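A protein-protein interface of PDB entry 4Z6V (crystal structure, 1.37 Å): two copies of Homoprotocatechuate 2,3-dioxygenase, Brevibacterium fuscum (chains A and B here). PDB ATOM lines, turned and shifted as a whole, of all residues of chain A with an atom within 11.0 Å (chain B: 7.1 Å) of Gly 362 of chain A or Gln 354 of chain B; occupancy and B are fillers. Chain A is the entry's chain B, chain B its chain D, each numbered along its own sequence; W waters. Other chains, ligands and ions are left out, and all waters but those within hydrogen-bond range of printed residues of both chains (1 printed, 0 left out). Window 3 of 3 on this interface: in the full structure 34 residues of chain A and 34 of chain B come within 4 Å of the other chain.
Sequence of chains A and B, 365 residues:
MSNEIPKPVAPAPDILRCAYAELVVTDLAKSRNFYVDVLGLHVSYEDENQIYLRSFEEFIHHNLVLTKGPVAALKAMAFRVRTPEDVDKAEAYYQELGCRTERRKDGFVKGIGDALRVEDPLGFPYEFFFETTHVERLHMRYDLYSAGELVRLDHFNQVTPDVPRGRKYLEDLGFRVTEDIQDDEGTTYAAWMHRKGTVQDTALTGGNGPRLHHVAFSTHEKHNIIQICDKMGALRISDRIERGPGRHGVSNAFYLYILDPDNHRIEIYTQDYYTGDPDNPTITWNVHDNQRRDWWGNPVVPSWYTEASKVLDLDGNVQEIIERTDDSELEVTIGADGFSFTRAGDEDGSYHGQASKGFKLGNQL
N of Lys 360 of chain B lies within hydrogen-bond range of O of Lys 360 of chain A, 2.8 Å away. N of Gly 362 of chain A sits at hydrogen-bond distance from O of Gly 358 of chain B.
The backbone carbonyl oxygen of Pro 302 of chain A sits at hydrogen-bond distance from the side-chain hydroxyl of Thr 306 of chain A (3.4 Å). The backbone carbonyl oxygen of Gly 353 of chain A sits at hydrogen-bond distance from the side-chain amino group of Lys 360 of chain A, 3.2 Å away.
Among the printed residues, merely in contact across the chains: Pro 299 of chain A with Phe 359 of chain B (3.6 Å), Val 300 of chain A with Phe 359 of chain B (3.98 Å), Val 301 of chain A with Lys 357 of chain B (3.3 Å), Val 301 of chain A with Phe 359 of chain B (3.5 Å), Pro 302 of chain A with Gly 358 of chain B (3.9 Å), Pro 302 of chain A with Phe 359 of chain B (3.9 Å), Gly 358 of chain A with Leu 361 of chain B (3.97 Å), Phe 359 of chain A with Phe 359 of chain B (3.7 Å), Phe 359 of chain A with Lys 360 of chain B (3.5 Å), Lys 360 of chain A with Phe 359 of chain B (3.4 Å), Lys 360 of chain A with Leu 361 of chain B (3.8 Å), Leu 361 of chain A with Lys 360 of chain B (3.4 Å), Gly 362 of chain A with Gln 354 of chain B (3.7 Å) and Gly 362 of chain A with Lys 360 of chain B (3.8 Å).
Of chain A, only Gly 362 (3.7 Å) comes within 4 Å of Gln 354 of chain B. Ile 334 of chain B touches none of the printed residues of chain A. No residue of chain A comes within 4 Å of Gly 335 of chain B. No residue of chain A comes within 4 Å of Ala 336 of chain B. No residue of chain A comes within 4 Å of Gly 338 of chain B. No residue of chain A comes within 4 Å of Ala 355 of chain B. No residue of chain A comes within 4 Å of Ser 356 of chain B. Gly 358 of chain B touches two residues of chain A. Printed residues of chain A within 4 Å of Lys 360 of chain B: Phe 359, Lys 360, Leu 361 and Gly 362. Of the printed residues of chain A, Phe 359 of chain B touches Pro 299, Val 300, Val 301, Pro 302, Phe 359 and Lys 360. Printed residues of chain B within 4 Å of Leu 361 of chain A: Lys 360 (3.4 Å). Of the printed residues of chain B, Pro 302 of chain A touches Gly 358 and Phe 359. Ile 334 of chain A touches none of the printed residues of chain B. The nearest residue of chain A that does not touch Gln 354 of chain B is Leu 361 of chain A (6.1 Å). The nearest printed residue of chain B that does not touch Leu 361 of chain A is Gly 358 of chain B (4.2 Å).
Along chain B the printed residues that touch a printed residue of chain A span positions 354 to 361. Of the 20 printed residues of chain A, 9 touch a printed residue of chain B. Printed residues of chain A that touch a printed residue of chain B: Pro 299, Val 300, Val 301, Pro 302, Gly 358, Phe 359, Lys 360, Leu 361 and Gly 362. Among the printed residues, no Asp or Glu carboxylate lies within 4 Å of a Lys or Arg side-chain nitrogen of the other chain.
Gly 358 of chain A touches Leu 361 of chain B, but with the chains exchanged Leu 361 of chain A does not touch Gly 358 of chain B (4.2 Å). Phe 359 of chain A touches Lys 360 of chain B, and with the chains exchanged Lys 360 of chain A touches Phe 359 of chain B. Lys 360 of chain A touches its own counterpart, Lys 360 of chain B. Lys 360 of chain A touches Leu 361 of chain B, and with the chains exchanged Leu 361 of chain A touches Lys 360 of chain B. Positions printed for both chains: 334, 335, 336, 353, 354, 355, 356, 358, 359, 360 and 361.
Water W1 bridges the backbone NH of Ser 303 of chain A and the backbone carbonyl oxygen of Lys 357 of chain B.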
ATOM      1  N   PRO A 299       3.531  11.160  -3.056  1.00  0.00           N
ATOM      2  CA  PRO A 299       4.138  12.278  -2.353  1.00  0.00           C
ATOM      3  C   PRO A 299       5.662  12.198  -2.376  1.00  0.00           C
ATOM      4  O   PRO A 299       6.228  11.112  -2.438  1.00  0.00           O
ATOM      5  CB  PRO A 299       3.600  12.127  -0.927  1.00  0.00           C
ATOM      6  CG  PRO A 299       3.327  10.667  -0.784  1.00  0.00           C
ATOM      7  CD  PRO A 299       2.820  10.255  -2.133  1.00  0.00           C
ATOM      8  N   VAL A 300       6.316  13.348  -2.370  1.00  0.00           N
ATOM      9  CA  VAL A 300       7.765  13.414  -2.371  1.00  0.00           C
ATOM     10  C   VAL A 300       8.225  13.432  -0.922  1.00  0.00           C
ATOM     11  O   VAL A 300       7.888  14.337  -0.168  1.00  0.00           O
ATOM     12  CB  VAL A 300       8.291  14.647  -3.146  1.00  0.00           C
ATOM     13  CG1 VAL A 300       9.813  14.703  -3.077  1.00  0.00           C
ATOM     14  CG2 VAL A 300       7.830  14.605  -4.597  1.00  0.00           C
ATOM     15  N   VAL A 301       9.004  12.417  -0.557  1.00  0.00           N
ATOM     16  CA  VAL A 301       9.470  12.262   0.812  1.00  0.00           C
ATOM     17  C   VAL A 301      10.315  13.487   1.234  1.00  0.00           C
ATOM     18  O   VAL A 301      11.114  13.992   0.441  1.00  0.00           O
ATOM     19  CB  VAL A 301      10.235  10.929   0.995  1.00  0.00           C
ATOM     20  CG1 VAL A 301       9.338   9.746   0.641  1.00  0.00           C
ATOM     21  CG2 VAL A 301      11.481  10.890   0.151  1.00  0.00           C
ATOM     22  N   PRO A 302      10.155  13.967   2.481  1.00  0.00           N
ATOM     23  CA  PRO A 302      10.829  15.234   2.834  1.00  0.00           C
ATOM     24  C   PRO A 302      12.354  15.172   2.756  1.00  0.00           C
ATOM     25  O   PRO A 302      12.989  16.164   2.400  1.00  0.00           O
ATOM     26  CB  PRO A 302      10.362  15.518   4.273  1.00  0.00           C
ATOM     27  CG  PRO A 302       9.136  14.672   4.453  1.00  0.00           C
ATOM     28  CD  PRO A 302       9.169  13.541   3.489  1.00  0.00           C
ATOM     29  N   SER A 303      12.938  14.005   3.020  1.00  0.00           N
ATOM     30  CA  SER A 303      14.383  13.855   2.874  1.00  0.00           C
ATOM     31  C   SER A 303      14.891  14.159   1.475  1.00  0.00           C
ATOM     32  O   SER A 303      16.032  14.588   1.312  1.00  0.00           O
ATOM     33  CB  SER A 303      14.870  12.450   3.270  1.00  0.00           C
ATOM     34  OG  SER A 303      14.398  11.439   2.398  1.00  0.00           O
ATOM     35  N   THR A 306      15.513  17.814   1.675  1.00  0.00           N
ATOM     36  CA  THR A 306      16.403  18.337   2.697  1.00  0.00           C
ATOM     37  C   THR A 306      17.811  17.732   2.731  1.00  0.00           C
ATOM     38  O   THR A 306      18.738  18.376   3.232  1.00  0.00           O
ATOM     39  CB  THR A 306      15.784  18.199   4.100  1.00  0.00           C
ATOM     40  OG1 THR A 306      15.678  16.820   4.438  1.00  0.00           O
ATOM     41  CG2 THR A 306      14.399  18.857   4.177  1.00  0.00           C
ATOM     42  N   LEU A 330       9.636  22.208  -0.707  1.00  0.00           N
ATOM     43  CA  LEU A 330       9.004  21.466   0.384  1.00  0.00           C
ATOM     44  C   LEU A 330       7.922  22.309   1.039  1.00  0.00           C
ATOM     45  O   LEU A 330       6.763  21.891   1.138  1.00  0.00           O
ATOM     46  CB  LEU A 330      10.048  20.991   1.407  1.00  0.00           C
ATOM     47  CG  LEU A 330       9.550  20.141   2.595  1.00  0.00           C
ATOM     48  CD1 LEU A 330      10.700  19.383   3.238  1.00  0.00           C
ATOM     49  CD2 LEU A 330       8.850  20.995   3.636  1.00  0.00           C
ATOM     50  N   GLU A 331       8.284  23.503   1.484  1.00  0.00           N
ATOM     51  CA  GLU A 331       7.327  24.306   2.253  1.00  0.00           C
ATOM     52  C   GLU A 331       6.085  24.667   1.456  1.00  0.00           C
ATOM     53  O   GLU A 331       4.955  24.579   1.949  1.00  0.00           O
ATOM     54  CB  GLU A 331       8.021  25.564   2.792  1.00  0.00           C
ATOM     55  CG  GLU A 331       9.046  25.296   3.893  1.00  0.00           C
ATOM     56  CD  GLU A 331       8.484  24.642   5.162  1.00  0.00           C
ATOM     57  OE1 GLU A 331       7.251  24.658   5.394  1.00  0.00           O
ATOM     58  OE2 GLU A 331       9.292  24.110   5.959  1.00  0.00           O
ATOM     59  N   ILE A 334       4.171  20.769   0.481  1.00  0.00           N
ATOM     60  CA  ILE A 334       3.784  19.765   1.483  1.00  0.00           C
ATOM     61  C   ILE A 334       3.920  20.245   2.929  1.00  0.00           C
ATOM     62  O   ILE A 334       3.548  19.530   3.871  1.00  0.00           O
ATOM     63  CB  ILE A 334       4.521  18.402   1.276  1.00  0.00           C
ATOM     64  CG1 ILE A 334       6.050  18.541   1.430  1.00  0.00           C
ATOM     65  CG2 ILE A 334       4.156  17.832  -0.078  1.00  0.00           C
ATOM     66  CD1 ILE A 334       6.804  17.206   1.405  1.00  0.00           C
ATOM     67  N   GLY A 335       4.446  21.454   3.101  1.00  0.00           N
ATOM     68  CA  GLY A 335       4.590  22.041   4.413  1.00  0.00           C
ATOM     69  C   GLY A 335       3.276  22.583   4.928  1.00  0.00           C
ATOM     70  O   GLY A 335       2.232  22.439   4.289  1.00  0.00           O
ATOM     71  N   ALA A 336       3.335  23.263   6.065  1.00  0.00           N
ATOM     72  CA  ALA A 336       2.125  23.639   6.803  1.00  0.00           C
ATOM     73  C   ALA A 336       1.220  24.618   6.059  1.00  0.00           C
ATOM     74  O   ALA A 336       0.004  24.579   6.213  1.00  0.00           O
ATOM     75  CB  ALA A 336       2.511  24.230   8.145  1.00  0.00           C
ATOM     76  N   GLY A 353      -1.766  22.064   3.087  1.00  0.00           N
ATOM     77  CA  GLY A 353      -0.993  21.865   4.295  1.00  0.00           C
ATOM     78  C   GLY A 353      -0.625  20.428   4.594  1.00  0.00           C
ATOM     79  O   GLY A 353      -0.414  20.067   5.751  1.00  0.00           O
ATOM     80  N   GLN A 354      -0.552  19.593   3.566  1.00  0.00           N
ATOM     81  CA  GLN A 354      -0.111  18.221   3.746  1.00  0.00           C
ATOM     82  C   GLN A 354       0.272  17.650   2.401  1.00  0.00           C
ATOM     83  O   GLN A 354       0.079  18.291   1.366  1.00  0.00           O
ATOM     84  CB  GLN A 354      -1.178  17.357   4.417  1.00  0.00           C
ATOM     85  CG  GLN A 354      -2.458  17.189   3.642  1.00  0.00           C
ATOM     86  CD  GLN A 354      -3.576  16.578   4.491  1.00  0.00           C
ATOM     87  OE1 GLN A 354      -4.739  16.624   4.098  1.00  0.00           O
ATOM     88  NE2 GLN A 354      -3.228  16.018   5.656  1.00  0.00           N
ATOM     89  N   ALA A 355       0.815  16.439   2.439  1.00  0.00           N
ATOM     90  CA  ALA A 355       1.208  15.728   1.252  1.00  0.00           C
ATOM     91  C   ALA A 355      -0.007  15.021   0.635  1.00  0.00           C
ATOM     92  O   ALA A 355      -1.088  14.959   1.238  1.00  0.00           O
ATOM     93  CB  ALA A 355       2.303  14.728   1.589  1.00  0.00           C
ATOM     94  N   SER A 356       0.179  14.510  -0.575  1.00  0.00           N
ATOM     95  CA  SER A 356      -0.836  13.682  -1.227  1.00  0.00           C
ATOM     96  C   SER A 356      -0.958  12.324  -0.566  1.00  0.00           C
ATOM     97  O   SER A 356      -0.097  11.916   0.244  1.00  0.00           O
ATOM     98  CB  SER A 356      -0.465  13.478  -2.694  1.00  0.00           C
ATOM     99  OG  SER A 356       0.844  12.948  -2.799  1.00  0.00           O
ATOM    100  N   GLY A 358      -2.739  10.948   1.666  1.00  0.00           N
ATOM    101  CA  GLY A 358      -3.103  10.706   3.054  1.00  0.00           C
ATOM    102  C   GLY A 358      -1.992  10.872   4.081  1.00  0.00           C
ATOM    103  O   GLY A 358      -2.157  10.488   5.235  1.00  0.00           O
ATOM    104  N   PHE A 359      -0.884  11.485   3.680  1.00  0.00           N
ATOM    105  CA  PHE A 359       0.273  11.653   4.546  1.00  0.00           C
ATOM    106  C   PHE A 359       0.550  13.122   4.881  1.00  0.00           C
ATOM    107  O   PHE A 359       0.131  14.029   4.161  1.00  0.00           O
ATOM    108  CB  PHE A 359       1.513  11.039   3.906  1.00  0.00           C
ATOM    109  CG  PHE A 359       1.423   9.550   3.736  1.00  0.00           C
ATOM    110  CD1 PHE A 359       1.336   8.709   4.831  1.00  0.00           C
ATOM    111  CD2 PHE A 359       1.408   8.986   2.455  1.00  0.00           C
ATOM    112  CE1 PHE A 359       1.254   7.326   4.647  1.00  0.00           C
ATOM    113  CE2 PHE A 359       1.332   7.622   2.275  1.00  0.00           C
ATOM    114  CZ  PHE A 359       1.244   6.799   3.370  1.00  0.00           C
ATOM    115  N   LYS A 360       1.253  13.311   6.000  1.00  0.00           N
ATOM    116  CA  LYS A 360       1.798  14.585   6.443  1.00  0.00           C
ATOM    117  C   LYS A 360       3.274  14.390   6.725  1.00  0.00           C
ATOM    118  O   LYS A 360       3.717  13.261   6.940  1.00  0.00           O
ATOM    119  CB  LYS A 360       1.128  15.024   7.759  1.00  0.00           C
ATOM    120  CG  LYS A 360      -0.026  15.967   7.590  1.00  0.00           C
ATOM    121  CD  LYS A 360      -0.608  16.332   8.956  1.00  0.00           C
ATOM    122  CE  LYS A 360      -1.755  17.331   8.833  1.00  0.00           C
ATOM    123  NZ  LYS A 360      -1.293  18.706   8.500  1.00  0.00           N
ATOM    124  N   LEU A 361       4.019  15.492   6.721  1.00  0.00           N
ATOM    125  CA  LEU A 361       5.421  15.518   7.144  1.00  0.00           C
ATOM    126  C   LEU A 361       5.569  14.870   8.532  1.00  0.00           C
ATOM    127  O   LEU A 361       4.844  15.234   9.443  1.00  0.00           O
ATOM    128  CB  LEU A 361       5.915  16.976   7.245  1.00  0.00           C
ATOM    129  CG  LEU A 361       6.051  17.894   6.038  1.00  0.00           C
ATOM    130  CD1 LEU A 361       6.516  19.274   6.489  1.00  0.00           C
ATOM    131  CD2 LEU A 361       7.036  17.317   5.050  1.00  0.00           C
ATOM    132  N   GLY A 362       6.506  13.928   8.700  1.00  0.00           N
ATOM    133  CA  GLY A 362       6.871  13.439  10.038  1.00  0.00           C
ATOM    134  C   GLY A 362       7.319  14.540  10.995  1.00  0.00           C
ATOM    135  O   GLY A 362       7.917  15.537  10.575  1.00  0.00           O
ATOM    136  N   THR B 333       0.992  -0.328  13.420  1.00  0.00           N
ATOM    137  CA  THR B 333       2.091  -0.168  12.477  1.00  0.00           C
ATOM    138  C   THR B 333       2.429   1.289  12.138  1.00  0.00           C
ATOM    139  O   THR B 333       3.612   1.633  12.087  1.00  0.00           O
ATOM    140  CB  THR B 333       1.847  -0.942  11.164  1.00  0.00           C
ATOM    141  OG1 THR B 333       0.717  -0.428  10.462  1.00  0.00           O
ATOM    142  CG2 THR B 333       1.651  -2.439  11.433  1.00  0.00           C
ATOM    143  N   ILE B 334       1.423   2.120  11.849  1.00  0.00           N
ATOM    144  CA  ILE B 334       1.675   3.495  11.364  1.00  0.00           C
ATOM    145  C   ILE B 334       1.031   4.602  12.187  1.00  0.00           C
ATOM    146  O   ILE B 334       1.266   5.796  11.913  1.00  0.00           O
ATOM    147  CB  ILE B 334       1.313   3.663   9.860  1.00  0.00           C
ATOM    148  CG1 ILE B 334      -0.175   3.434   9.586  1.00  0.00           C
ATOM    149  CG2 ILE B 334       2.156   2.715   9.017  1.00  0.00           C
ATOM    150  CD1 ILE B 334      -0.619   3.789   8.182  1.00  0.00           C
ATOM    151  N   GLY B 335       0.258   4.239  13.210  1.00  0.00           N
ATOM    152  CA  GLY B 335      -0.347   5.249  14.068  1.00  0.00           C
ATOM    153  C   GLY B 335       0.683   5.778  15.054  1.00  0.00           C
ATOM    154  O   GLY B 335       1.842   5.350  15.042  1.00  0.00           O
ATOM    155  N   ALA B 336       0.273   6.717  15.903  1.00  0.00           N
ATOM    156  CA  ALA B 336       1.212   7.366  16.817  1.00  0.00           C
ATOM    157  C   ALA B 336       1.869   6.373  17.812  1.00  0.00           C
ATOM    158  O   ALA B 336       2.973   6.633  18.286  1.00  0.00           O
ATOM    159  CB  ALA B 336       0.534   8.516  17.562  1.00  0.00           C
ATOM    160  N   ASP B 337       1.213   5.247  18.117  1.00  0.00           N
ATOM    161  CA  ASP B 337       1.788   4.223  19.002  1.00  0.00           C
ATOM    162  C   ASP B 337       2.272   2.996  18.235  1.00  0.00           C
ATOM    163  O   ASP B 337       2.578   1.966  18.844  1.00  0.00           O
ATOM    164  CB  ASP B 337       0.744   3.755  20.018  1.00  0.00           C
ATOM    165  CG  ASP B 337       0.395   4.823  21.032  1.00  0.00           C
ATOM    166  OD1 ASP B 337       1.266   5.639  21.349  1.00  0.00           O
ATOM    167  OD2 ASP B 337      -0.748   4.830  21.506  1.00  0.00           O
ATOM    168  N   GLY B 338       2.318   3.094  16.909  1.00  0.00           N
ATOM    169  CA  GLY B 338       2.660   1.959  16.057  1.00  0.00           C
ATOM    170  C   GLY B 338       4.154   1.832  15.884  1.00  0.00           C
ATOM    171  O   GLY B 338       4.912   2.744  16.214  1.00  0.00           O
ATOM    172  N   PHE B 339       4.579   0.714  15.320  1.00  0.00           N
ATOM    173  CA  PHE B 339       5.939   0.609  14.837  1.00  0.00           C
ATOM    174  C   PHE B 339       6.025  -0.423  13.748  1.00  0.00           C
ATOM    175  O   PHE B 339       5.178  -1.317  13.622  1.00  0.00           O
ATOM    176  CB  PHE B 339       6.916   0.308  15.974  1.00  0.00           C
ATOM    177  CG  PHE B 339       6.955  -1.123  16.383  1.00  0.00           C
ATOM    178  CD1 PHE B 339       6.061  -1.603  17.327  1.00  0.00           C
ATOM    179  CD2 PHE B 339       7.925  -1.975  15.878  1.00  0.00           C
ATOM    180  CE1 PHE B 339       6.098  -2.931  17.736  1.00  0.00           C
ATOM    181  CE2 PHE B 339       7.983  -3.304  16.286  1.00  0.00           C
ATOM    182  CZ  PHE B 339       7.057  -3.782  17.210  1.00  0.00           C
ATOM    183  N   SER B 340       7.065  -0.297  12.949  1.00  0.00           N
ATOM    184  CA  SER B 340       7.405  -1.336  11.989  1.00  0.00           C
ATOM    185  C   SER B 340       8.935  -1.402  11.872  1.00  0.00           C
ATOM    186  O   SER B 340       9.644  -0.480  12.250  1.00  0.00           O
ATOM    187  CB  SER B 340       6.753  -1.078  10.610  1.00  0.00           C
ATOM    188  OG  SER B 340       7.313   0.038   9.964  1.00  0.00           O
ATOM    189  N   SER B 350      13.888   1.077  11.401  1.00  0.00           N
ATOM    190  CA  SER B 350      12.602   0.935  12.060  1.00  0.00           C
ATOM    191  C   SER B 350      11.900   2.281  12.205  1.00  0.00           C
ATOM    192  O   SER B 350      12.533   3.345  12.196  1.00  0.00           O
ATOM    193  CB  SER B 350      12.764   0.281  13.429  1.00  0.00           C
ATOM    194  OG  SER B 350      13.364   1.159  14.364  1.00  0.00           O
ATOM    195  N   TYR B 351      10.582   2.216  12.335  1.00  0.00           N
ATOM    196  CA  TYR B 351       9.722   3.403  12.313  1.00  0.00           C
ATOM    197  C   TYR B 351       8.821   3.330  13.524  1.00  0.00           C
ATOM    198  O   TYR B 351       8.212   2.297  13.783  1.00  0.00           O
ATOM    199  CB  TYR B 351       8.914   3.467  11.010  1.00  0.00           C
ATOM    200  CG  TYR B 351       9.797   3.388   9.808  1.00  0.00           C
ATOM    201  CD1 TYR B 351      10.607   4.463   9.453  1.00  0.00           C
ATOM    202  CD2 TYR B 351       9.921   2.211   9.102  1.00  0.00           C
ATOM    203  CE1 TYR B 351      11.454   4.379   8.357  1.00  0.00           C
ATOM    204  CE2 TYR B 351      10.781   2.108   8.034  1.00  0.00           C
ATOM    205  CZ  TYR B 351      11.539   3.193   7.655  1.00  0.00           C
ATOM    206  OH  TYR B 351      12.379   3.075   6.579  1.00  0.00           O
ATOM    207  N   HIS B 352       8.789   4.410  14.300  1.00  0.00           N
ATOM    208  CA  HIS B 352       8.009   4.437  15.530  1.00  0.00           C
ATOM    209  C   HIS B 352       7.117   5.663  15.516  1.00  0.00           C
ATOM    210  O   HIS B 352       7.602   6.794  15.420  1.00  0.00           O
ATOM    211  CB  HIS B 352       8.917   4.472  16.768  1.00  0.00           C
ATOM    212  CG  HIS B 352       9.867   3.320  16.845  1.00  0.00           C
ATOM    213  ND1 HIS B 352       9.594   2.175  17.559  1.00  0.00           N
ATOM    214  CD2 HIS B 352      11.084   3.133  16.286  1.00  0.00           C
ATOM    215  CE1 HIS B 352      10.606   1.334  17.442  1.00  0.00           C
ATOM    216  NE2 HIS B 352      11.526   1.894  16.678  1.00  0.00           N
ATOM    217  N   GLY B 353       5.814   5.434  15.595  1.00  0.00           N
ATOM    218  CA  GLY B 353       4.842   6.519  15.668  1.00  0.00           C
ATOM    219  C   GLY B 353       4.585   7.207  14.344  1.00  0.00           C
ATOM    220  O   GLY B 353       3.968   8.282  14.289  1.00  0.00           O
ATOM    221  N   GLN B 354       5.059   6.584  13.268  1.00  0.00           N
ATOM    222  CA  GLN B 354       4.836   7.099  11.935  1.00  0.00           C
ATOM    223  C   GLN B 354       5.104   6.028  10.921  1.00  0.00           C
ATOM    224  O   GLN B 354       5.567   4.923  11.274  1.00  0.00           O
ATOM    225  CB  GLN B 354       5.672   8.343  11.660  1.00  0.00           C
ATOM    226  CG  GLN B 354       7.174   8.157  11.593  1.00  0.00           C
ATOM    227  CD  GLN B 354       7.893   9.498  11.399  1.00  0.00           C
ATOM    228  OE1 GLN B 354       8.728   9.659  10.506  1.00  0.00           O
ATOM    229  NE2 GLN B 354       7.534  10.474  12.215  1.00  0.00           N
ATOM    230  N   ALA B 355       4.760   6.341   9.673  1.00  0.00           N
ATOM    231  CA  ALA B 355       4.969   5.417   8.590  1.00  0.00           C
ATOM    232  C   ALA B 355       6.408   5.439   8.100  1.00  0.00           C
ATOM    233  O   ALA B 355       7.238   6.238   8.534  1.00  0.00           O
ATOM    234  CB  ALA B 355       3.989   5.700   7.471  1.00  0.00           C
ATOM    235  N   SER B 356       6.718   4.517   7.214  1.00  0.00           N
ATOM    236  CA  SER B 356       8.034   4.484   6.619  1.00  0.00           C
ATOM    237  C   SER B 356       8.244   5.700   5.737  1.00  0.00           C
ATOM    238  O   SER B 356       7.276   6.424   5.397  1.00  0.00           O
ATOM    239  CB  SER B 356       8.182   3.199   5.818  1.00  0.00           C
ATOM    240  OG  SER B 356       7.090   3.051   4.937  1.00  0.00           O
ATOM    241  N   LYS B 357       9.514   5.900   5.366  1.00  0.00           N
ATOM    242  CA  LYS B 357       9.938   6.854   4.338  1.00  0.00           C
ATOM    243  C   LYS B 357       9.689   8.326   4.706  1.00  0.00           C
ATOM    244  O   LYS B 357       9.764   9.190   3.843  1.00  0.00           O
ATOM    245  CB  LYS B 357       9.336   6.546   2.930  1.00  0.00           C
ATOM    246  CG  LYS B 357       9.257   5.079   2.516  1.00  0.00           C
ATOM    247  CD  LYS B 357      10.556   4.533   1.986  1.00  0.00           C
ATOM    248  CE  LYS B 357      10.411   3.179   1.307  1.00  0.00           C
ATOM    249  NZ  LYS B 357      11.562   2.279   1.640  1.00  0.00           N
ATOM    250  N   GLY B 358       9.385   8.631   5.966  1.00  0.00           N
ATOM    251  CA  GLY B 358       9.384  10.024   6.438  1.00  0.00           C
ATOM    252  C   GLY B 358       8.030  10.686   6.620  1.00  0.00           C
ATOM    253  O   GLY B 358       7.955  11.904   6.866  1.00  0.00           O
ATOM    254  N   PHE B 359       6.964   9.909   6.494  1.00  0.00           N
ATOM    255  CA  PHE B 359       5.594  10.426   6.609  1.00  0.00           C
ATOM    256  C   PHE B 359       4.945  10.033   7.934  1.00  0.00           C
ATOM    257  O   PHE B 359       5.170   8.928   8.416  1.00  0.00           O
ATOM    258  CB  PHE B 359       4.741   9.886   5.454  1.00  0.00           C
ATOM    259  CG  PHE B 359       5.186  10.372   4.101  1.00  0.00           C
ATOM    260  CD1 PHE B 359       5.170  11.725   3.797  1.00  0.00           C
ATOM    261  CD2 PHE B 359       5.622   9.462   3.128  1.00  0.00           C
ATOM    262  CE1 PHE B 359       5.597  12.180   2.544  1.00  0.00           C
ATOM    263  CE2 PHE B 359       6.039   9.902   1.891  1.00  0.00           C
ATOM    264  CZ  PHE B 359       6.024  11.266   1.594  1.00  0.00           C
ATOM    265  N   LYS B 360       4.117  10.918   8.494  1.00  0.00           N
ATOM    266  CA  LYS B 360       3.116  10.505   9.488  1.00  0.00           C
ATOM    267  C   LYS B 360       1.711  10.552   8.896  1.00  0.00           C
ATOM    268  O   LYS B 360       1.519  10.989   7.754  1.00  0.00           O
ATOM    269  CB  LYS B 360       3.227  11.361  10.751  1.00  0.00           C
ATOM    270  CG  LYS B 360       2.744  12.781  10.598  1.00  0.00           C
ATOM    271  CD  LYS B 360       2.808  13.525  11.908  1.00  0.00           C
ATOM    272  CE  LYS B 360       2.230  14.922  11.734  1.00  0.00           C
ATOM    273  NZ  LYS B 360       2.094  15.657  13.026  1.00  0.00           N
ATOM    274  N   LEU B 361       0.732  10.095   9.669  1.00  0.00           N
ATOM    275  CA  LEU B 361      -0.646  10.065   9.189  1.00  0.00           C
ATOM    276  C   LEU B 361      -1.111  11.494   8.934  1.00  0.00           C
ATOM    277  O   LEU B 361      -0.817  12.398   9.736  1.00  0.00           O
ATOM    278  CB  LEU B 361      -1.564   9.386  10.207  1.00  0.00           C
ATOM    279  CG  LEU B 361      -1.320   7.924  10.587  1.00  0.00           C
ATOM    280  CD1 LEU B 361      -2.365   7.499  11.607  1.00  0.00           C
ATOM    281  CD2 LEU B 361      -1.399   7.015   9.389  1.00  0.00           C
HETATM  282  O   HOH W   1      11.872  11.570   4.407  1.00  0.00           O
